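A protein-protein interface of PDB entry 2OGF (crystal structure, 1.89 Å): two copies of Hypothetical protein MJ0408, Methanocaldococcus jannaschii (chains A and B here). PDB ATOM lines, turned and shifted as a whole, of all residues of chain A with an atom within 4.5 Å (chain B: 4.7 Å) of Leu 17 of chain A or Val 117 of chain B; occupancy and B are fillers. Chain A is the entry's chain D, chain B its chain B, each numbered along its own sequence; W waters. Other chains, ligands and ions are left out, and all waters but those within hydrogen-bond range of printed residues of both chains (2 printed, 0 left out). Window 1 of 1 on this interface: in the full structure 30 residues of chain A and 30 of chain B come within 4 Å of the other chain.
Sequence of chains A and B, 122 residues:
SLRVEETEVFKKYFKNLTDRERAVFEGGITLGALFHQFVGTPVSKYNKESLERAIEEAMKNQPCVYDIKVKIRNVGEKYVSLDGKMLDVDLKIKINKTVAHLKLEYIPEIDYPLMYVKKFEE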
ATOM      1  N   PHE A  14       5.575  26.407 -10.132  1.00  0.00           N
ATOM      2  CA  PHE A  14       4.130  26.647  -9.963  1.00  0.00           C
ATOM      3  C   PHE A  14       3.586  27.957 -10.537  1.00  0.00           C
ATOM      4  O   PHE A  14       2.441  28.338 -10.268  1.00  0.00           O
ATOM      5  CB  PHE A  14       3.719  26.455  -8.497  1.00  0.00           C
ATOM      6  CG  PHE A  14       4.058  25.089  -7.978  1.00  0.00           C
ATOM      7  CD1 PHE A  14       3.213  24.015  -8.222  1.00  0.00           C
ATOM      8  CD2 PHE A  14       5.266  24.861  -7.309  1.00  0.00           C
ATOM      9  CE1 PHE A  14       3.552  22.730  -7.779  1.00  0.00           C
ATOM     10  CE2 PHE A  14       5.611  23.581  -6.870  1.00  0.00           C
ATOM     11  CZ  PHE A  14       4.761  22.528  -7.097  1.00  0.00           C
ATOM     12  N   LYS A  15       4.399  28.611 -11.362  1.00  0.00           N
ATOM     13  CA  LYS A  15       4.004  29.846 -12.044  1.00  0.00           C
ATOM     14  C   LYS A  15       2.840  29.640 -13.027  1.00  0.00           C
ATOM     15  O   LYS A  15       2.184  30.599 -13.413  1.00  0.00           O
ATOM     16  CB  LYS A  15       5.205  30.440 -12.792  1.00  0.00           C
ATOM     17  CG  LYS A  15       6.471  30.649 -11.946  1.00  0.00           C
ATOM     18  CD  LYS A  15       7.459  31.615 -12.619  1.00  0.00           C
ATOM     19  CE  LYS A  15       7.599  31.389 -14.142  1.00  0.00           C
ATOM     20  NZ  LYS A  15       7.988  32.639 -14.893  1.00  0.00           N
ATOM     21  N   ASN A  16       2.606  28.397 -13.447  1.00  0.00           N
ATOM     22  CA  ASN A  16       1.507  28.096 -14.363  1.00  0.00           C
ATOM     23  C   ASN A  16       0.127  27.843 -13.727  1.00  0.00           C
ATOM     24  O   ASN A  16      -0.842  27.602 -14.446  1.00  0.00           O
ATOM     25  CB  ASN A  16       1.897  26.966 -15.334  1.00  0.00           C
ATOM     26  CG  ASN A  16       2.004  25.602 -14.660  1.00  0.00           C
ATOM     27  OD1 ASN A  16       2.136  25.504 -13.444  1.00  0.00           O
ATOM     28  ND2 ASN A  16       1.969  24.544 -15.469  1.00  0.00           N
ATOM     29  N   LEU A  17       0.030  27.928 -12.399  1.00  0.00           N
ATOM     30  CA  LEU A  17      -1.245  27.682 -11.700  1.00  0.00           C
ATOM     31  C   LEU A  17      -1.785  28.906 -10.960  1.00  0.00           C
ATOM     32  O   LEU A  17      -1.012  29.751 -10.483  1.00  0.00           O
ATOM     33  CB  LEU A  17      -1.114  26.515 -10.700  1.00  0.00           C
ATOM     34  CG  LEU A  17      -0.553  25.151 -11.139  1.00  0.00           C
ATOM     35  CD1 LEU A  17      -0.503  24.218  -9.933  1.00  0.00           C
ATOM     36  CD2 LEU A  17      -1.322  24.476 -12.295  1.00  0.00           C
ATOM     37  N   THR A  18      -3.108  28.980 -10.849  1.00  0.00           N
ATOM     38  CA  THR A  18      -3.766  29.989 -10.027  1.00  0.00           C
ATOM     39  C   THR A  18      -3.575  29.551  -8.581  1.00  0.00           C
ATOM     40  O   THR A  18      -3.228  28.397  -8.322  1.00  0.00           O
ATOM     41  CB  THR A  18      -5.286  30.082 -10.321  1.00  0.00           C
ATOM     42  OG1 THR A  18      -5.936  28.894  -9.856  1.00  0.00           O
ATOM     43  CG2 THR A  18      -5.563  30.234 -11.816  1.00  0.00           C
ATOM     44  N   ASP A  19      -3.809  30.460  -7.641  1.00  0.00           N
ATOM     45  CA  ASP A  19      -3.684  30.120  -6.237  1.00  0.00           C
ATOM     46  C   ASP A  19      -4.690  29.045  -5.806  1.00  0.00           C
ATOM     47  O   ASP A  19      -4.369  28.203  -4.973  1.00  0.00           O
ATOM     48  CB  ASP A  19      -3.806  31.380  -5.367  1.00  0.00           C
ATOM     49  CG  ASP A  19      -2.615  32.331  -5.531  1.00  0.00           C
ATOM     50  OD1 ASP A  19      -1.647  32.002  -6.248  1.00  0.00           O
ATOM     51  OD2 ASP A  19      -2.655  33.421  -4.935  1.00  0.00           O
ATOM     52  N   GLU A  21      -5.956  26.673  -7.831  1.00  0.00           N
ATOM     53  CA  GLU A  21      -5.410  25.452  -8.418  1.00  0.00           C
ATOM     54  C   GLU A  21      -4.272  24.901  -7.565  1.00  0.00           C
ATOM     55  O   GLU A  21      -4.283  23.724  -7.212  1.00  0.00           O
ATOM     56  CB  GLU A  21      -4.941  25.675  -9.865  1.00  0.00           C
ATOM     57  CG  GLU A  21      -6.087  25.756 -10.896  1.00  0.00           C
ATOM     58  CD  GLU A  21      -5.695  26.470 -12.188  1.00  0.00           C
ATOM     59  OE1 GLU A  21      -4.502  26.771 -12.400  1.00  0.00           O
ATOM     60  OE2 GLU A  21      -6.606  26.730 -13.002  1.00  0.00           O
ATOM     61  N   ARG A  22      -3.306  25.747  -7.211  1.00  0.00           N
ATOM     62  CA  ARG A  22      -2.219  25.295  -6.316  1.00  0.00           C
ATOM     63  C   ARG A  22      -2.735  24.731  -4.990  1.00  0.00           C
ATOM     64  O   ARG A  22      -2.220  23.715  -4.537  1.00  0.00           O
ATOM     65  CB  ARG A  22      -1.196  26.397  -6.005  1.00  0.00           C
ATOM     66  CG  ARG A  22      -0.201  26.725  -7.107  1.00  0.00           C
ATOM     67  CD  ARG A  22       0.893  27.667  -6.569  1.00  0.00           C
ATOM     68  NE  ARG A  22       1.735  26.996  -5.578  1.00  0.00           N
ATOM     69  CZ  ARG A  22       2.596  27.603  -4.760  1.00  0.00           C
ATOM     70  NH1 ARG A  22       2.748  28.931  -4.770  1.00  0.00           N
ATOM     71  NH2 ARG A  22       3.302  26.879  -3.910  1.00  0.00           N
ATOM     72  N   PHE A  25      -4.354  21.389  -5.544  1.00  0.00           N
ATOM     73  CA  PHE A  25      -3.299  20.433  -5.909  1.00  0.00           C
ATOM     74  C   PHE A  25      -2.550  19.981  -4.649  1.00  0.00           C
ATOM     75  O   PHE A  25      -2.408  18.776  -4.403  1.00  0.00           O
ATOM     76  CB  PHE A  25      -2.340  21.078  -6.914  1.00  0.00           C
ATOM     77  CG  PHE A  25      -1.104  20.247  -7.239  1.00  0.00           C
ATOM     78  CD1 PHE A  25      -1.215  19.025  -7.913  1.00  0.00           C
ATOM     79  CD2 PHE A  25       0.167  20.716  -6.904  1.00  0.00           C
ATOM     80  CE1 PHE A  25      -0.065  18.279  -8.245  1.00  0.00           C
ATOM     81  CE2 PHE A  25       1.330  19.983  -7.224  1.00  0.00           C
ATOM     82  CZ  PHE A  25       1.219  18.771  -7.894  1.00  0.00           C
ATOM     83  N   VAL B  24      -6.357  19.071 -11.262  1.00  0.00           N
ATOM     84  CA  VAL B  24      -5.125  19.161 -10.482  1.00  0.00           C
ATOM     85  C   VAL B  24      -5.312  18.607  -9.062  1.00  0.00           C
ATOM     86  O   VAL B  24      -4.383  18.015  -8.518  1.00  0.00           O
ATOM     87  CB  VAL B  24      -4.471  20.576 -10.484  1.00  0.00           C
ATOM     88  CG1 VAL B  24      -4.169  21.043 -11.932  1.00  0.00           C
ATOM     89  CG2 VAL B  24      -5.307  21.593  -9.730  1.00  0.00           C
ATOM     90  N   HIS B 101      -1.597  17.490 -17.239  1.00  0.00           N
ATOM     91  CA  HIS B 101      -0.404  16.658 -17.313  1.00  0.00           C
ATOM     92  C   HIS B 101       0.457  17.000 -16.102  1.00  0.00           C
ATOM     93  O   HIS B 101       0.885  18.144 -15.940  1.00  0.00           O
ATOM     94  CB  HIS B 101       0.383  16.890 -18.610  1.00  0.00           C
ATOM     95  CG  HIS B 101      -0.386  16.589 -19.867  1.00  0.00           C
ATOM     96  ND1 HIS B 101       0.048  15.674 -20.803  1.00  0.00           N
ATOM     97  CD2 HIS B 101      -1.550  17.093 -20.347  1.00  0.00           C
ATOM     98  CE1 HIS B 101      -0.819  15.620 -21.798  1.00  0.00           C
ATOM     99  NE2 HIS B 101      -1.798  16.470 -21.546  1.00  0.00           N
ATOM    100  N   LEU B 102       0.689  16.015 -15.242  1.00  0.00           N
ATOM    101  CA  LEU B 102       1.443  16.262 -14.008  1.00  0.00           C
ATOM    102  C   LEU B 102       2.724  15.450 -13.997  1.00  0.00           C
ATOM    103  O   LEU B 102       2.831  14.433 -14.692  1.00  0.00           O
ATOM    104  CB  LEU B 102       0.607  15.945 -12.769  1.00  0.00           C
ATOM    105  CG  LEU B 102      -0.783  16.588 -12.648  1.00  0.00           C
ATOM    106  CD1 LEU B 102      -1.872  15.644 -13.154  1.00  0.00           C
ATOM    107  CD2 LEU B 102      -1.040  16.916 -11.231  1.00  0.00           C
ATOM    108  N   TYR B 116       4.427  18.445  -9.565  1.00  0.00           N
ATOM    109  CA  TYR B 116       3.946  19.695 -10.172  1.00  0.00           C
ATOM    110  C   TYR B 116       3.119  19.443 -11.433  1.00  0.00           C
ATOM    111  O   TYR B 116       3.001  18.295 -11.887  1.00  0.00           O
ATOM    112  CB  TYR B 116       5.118  20.664 -10.451  1.00  0.00           C
ATOM    113  CG  TYR B 116       6.110  20.210 -11.519  1.00  0.00           C
ATOM    114  CD1 TYR B 116       6.012  20.677 -12.837  1.00  0.00           C
ATOM    115  CD2 TYR B 116       7.163  19.344 -11.207  1.00  0.00           C
ATOM    116  CE1 TYR B 116       6.942  20.276 -13.830  1.00  0.00           C
ATOM    117  CE2 TYR B 116       8.085  18.938 -12.183  1.00  0.00           C
ATOM    118  CZ  TYR B 116       7.975  19.415 -13.484  1.00  0.00           C
ATOM    119  OH  TYR B 116       8.896  19.009 -14.435  1.00  0.00           O
ATOM    120  N   VAL B 117       2.549  20.515 -11.983  1.00  0.00           N
ATOM    121  CA  VAL B 117       1.753  20.438 -13.207  1.00  0.00           C
ATOM    122  C   VAL B 117       2.566  20.966 -14.393  1.00  0.00           C
ATOM    123  O   VAL B 117       3.002  22.125 -14.390  1.00  0.00           O
ATOM    124  CB  VAL B 117       0.424  21.215 -13.089  1.00  0.00           C
ATOM    125  CG1 VAL B 117      -0.385  21.125 -14.398  1.00  0.00           C
ATOM    126  CG2 VAL B 117      -0.426  20.716 -11.893  1.00  0.00           C
ATOM    127  N   LYS B 118       2.762  20.104 -15.387  1.00  0.00           N
ATOM    128  CA  LYS B 118       3.449  20.449 -16.631  1.00  0.00           C
ATOM    129  C   LYS B 118       2.627  21.404 -17.474  1.00  0.00           C
ATOM    130  O   LYS B 118       3.075  22.501 -17.822  1.00  0.00           O
ATOM    131  CB  LYS B 118       3.710  19.197 -17.468  1.00  0.00           C
ATOM    132  CG  LYS B 118       4.901  18.379 -17.054  1.00  0.00           C
ATOM    133  CD  LYS B 118       6.204  18.952 -17.589  1.00  0.00           C
ATOM    134  CE  LYS B 118       7.373  18.114 -17.099  1.00  0.00           C
ATOM    135  NZ  LYS B 118       8.690  18.715 -17.460  1.00  0.00           N
ATOM    136  N   LYS B 119       1.416  20.973 -17.797  1.00  0.00           N
ATOM    137  CA  LYS B 119       0.581  21.667 -18.754  1.00  0.00           C
ATOM    138  C   LYS B 119      -0.852  21.182 -18.629  1.00  0.00           C
ATOM    139  O   LYS B 119      -1.115  20.129 -18.022  1.00  0.00           O
ATOM    140  CB  LYS B 119       1.101  21.436 -20.191  1.00  0.00           C
ATOM    141  CG  LYS B 119       0.906  20.033 -20.747  1.00  0.00           C
ATOM    142  CD  LYS B 119       1.683  19.847 -22.052  1.00  0.00           C
ATOM    143  CE  LYS B 119       1.195  18.626 -22.822  1.00  0.00           C
ATOM    144  NZ  LYS B 119       1.830  18.530 -24.179  1.00  0.00           N
ATOM    145  N   PHE B 120      -1.763  21.967 -19.194  1.00  0.00           N
ATOM    146  CA  PHE B 120      -3.132  21.546 -19.434  1.00  0.00           C
ATOM    147  C   PHE B 120      -3.354  21.397 -20.930  1.00  0.00           C
ATOM    148  O   PHE B 120      -2.782  22.142 -21.730  1.00  0.00           O
ATOM    149  CB  PHE B 120      -4.124  22.574 -18.894  1.00  0.00           C
ATOM    150  CG  PHE B 120      -4.065  22.757 -17.405  1.00  0.00           C
ATOM    151  CD1 PHE B 120      -4.880  21.999 -16.565  1.00  0.00           C
ATOM    152  CD2 PHE B 120      -3.203  23.696 -16.842  1.00  0.00           C
ATOM    153  CE1 PHE B 120      -4.838  22.176 -15.185  1.00  0.00           C
ATOM    154  CE2 PHE B 120      -3.150  23.878 -15.463  1.00  0.00           C
ATOM    155  CZ  PHE B 120      -3.975  23.114 -14.632  1.00  0.00           C
HETATM  156  O   HOH W   1       2.527  25.485 -18.437  1.00  0.00           O
HETATM  157  O   HOH W   2       2.697  23.423 -11.439  1.00  0.00           O
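The backbone carbonyl oxygen of Val 117 of chain B lies within hydrogen-bond range of the side-chain amide nitrogen of Asn 16 of chain A (2.8 Å). The side-chain amide nitrogen of Asn 16 of chain A lies within hydrogen-bond range of the backbone carbonyl oxygen of Lys 118 of chain B (3.3 Å).
O of His 101 of chain B sits at hydrogen-bond distance from N of Lys 118 of chain B, at 2.8 Å. NZ of Lys 118 of chain B lies within hydrogen-bond range of OH of Tyr 116 of chain B (3.0 Å). The side-chain hydroxyl of Thr 18 of chain A lies within hydrogen-bond range of the backbone NH of Glu 21 of chain A, at 3.0 Å.
Among the printed residues, merely in contact across the chains: Phe 14 of chain A with Tyr 116 of chain B, Leu 17 of chain A with Val 117 of chain B, Leu 17 of chain A with Phe 120 of chain B, Glu 21 of chain A with Val 24 of chain B, Phe 25 of chain A with Val 24 of chain B, Phe 25 of chain A with Leu 102 of chain B and Phe 25 of chain A with Tyr 116 of chain B.
Printed residues of chain B within 4 Å of Leu 17 of chain A: Val 117 and Phe 120. Of chain A, only Asn 16 (2.8 Å) and Leu 17 (3.8 Å) come within 4 Å of Val 117 of chain B. Printed residues of chain B within 4 Å of Phe 14 of chain A: Tyr 116. Of the printed residues of chain A, Val 24 of chain B touches Glu 21 (3.5 Å) and Phe 25 (3.4 Å). Of the printed residues of chain A, Phe 120 of chain B touches Leu 17 (3.7 Å). Of the printed residues of chain B, Glu 21 of chain A touches Val 24. Of the printed residues of chain B, Phe 25 of chain A touches Val 24, Leu 102 and Tyr 116. Asp 19 of chain A touches none of the printed residues of chain B. The nearest residue of chain B that does not touch Leu 17 of chain A is Val 24 of chain B (4.5 Å). The nearest printed residue of chain A that does not touch Tyr 116 of chain B is Leu 17 of chain A (6.2 Å).
Hydrophobic or aromatic side chains of chain A within 4 Å of the printed part of chain B: Phe 14, Leu 17 and Phe 25. Printed residues of chain B that touch a printed residue of chain A: Val 24, Leu 102, Tyr 116, Val 117, Lys 118 and Phe 120. Hydrophobic or aromatic side chains of chain B that line the printed part of chain A: Val 24, Leu 102, Tyr 116, Val 117 and Phe 120. Among the printed residues, no Asp or Glu carboxylate lies within 4 Å of a Lys or Arg side-chain nitrogen of the other chain.
No position is printed for both chains. Of the 9 pairs that touch across the chains among the printed residues, none has its exchanged pair printed and touching as well.
Water W2 lies within hydrogen-bond range of the side-chain amide oxygen (OD1) of Asn 16 of chain A (2.9 Å) and the backbone NH (N) of Val 117 of chain B (3.0 Å). Water W1 lies within hydrogen-bond range of the backbone carbonyl oxygen of Lys 118 of chain B (3.1 Å) and the side-chain amide nitrogen of Asn 16 of chain A (3.2 Å).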
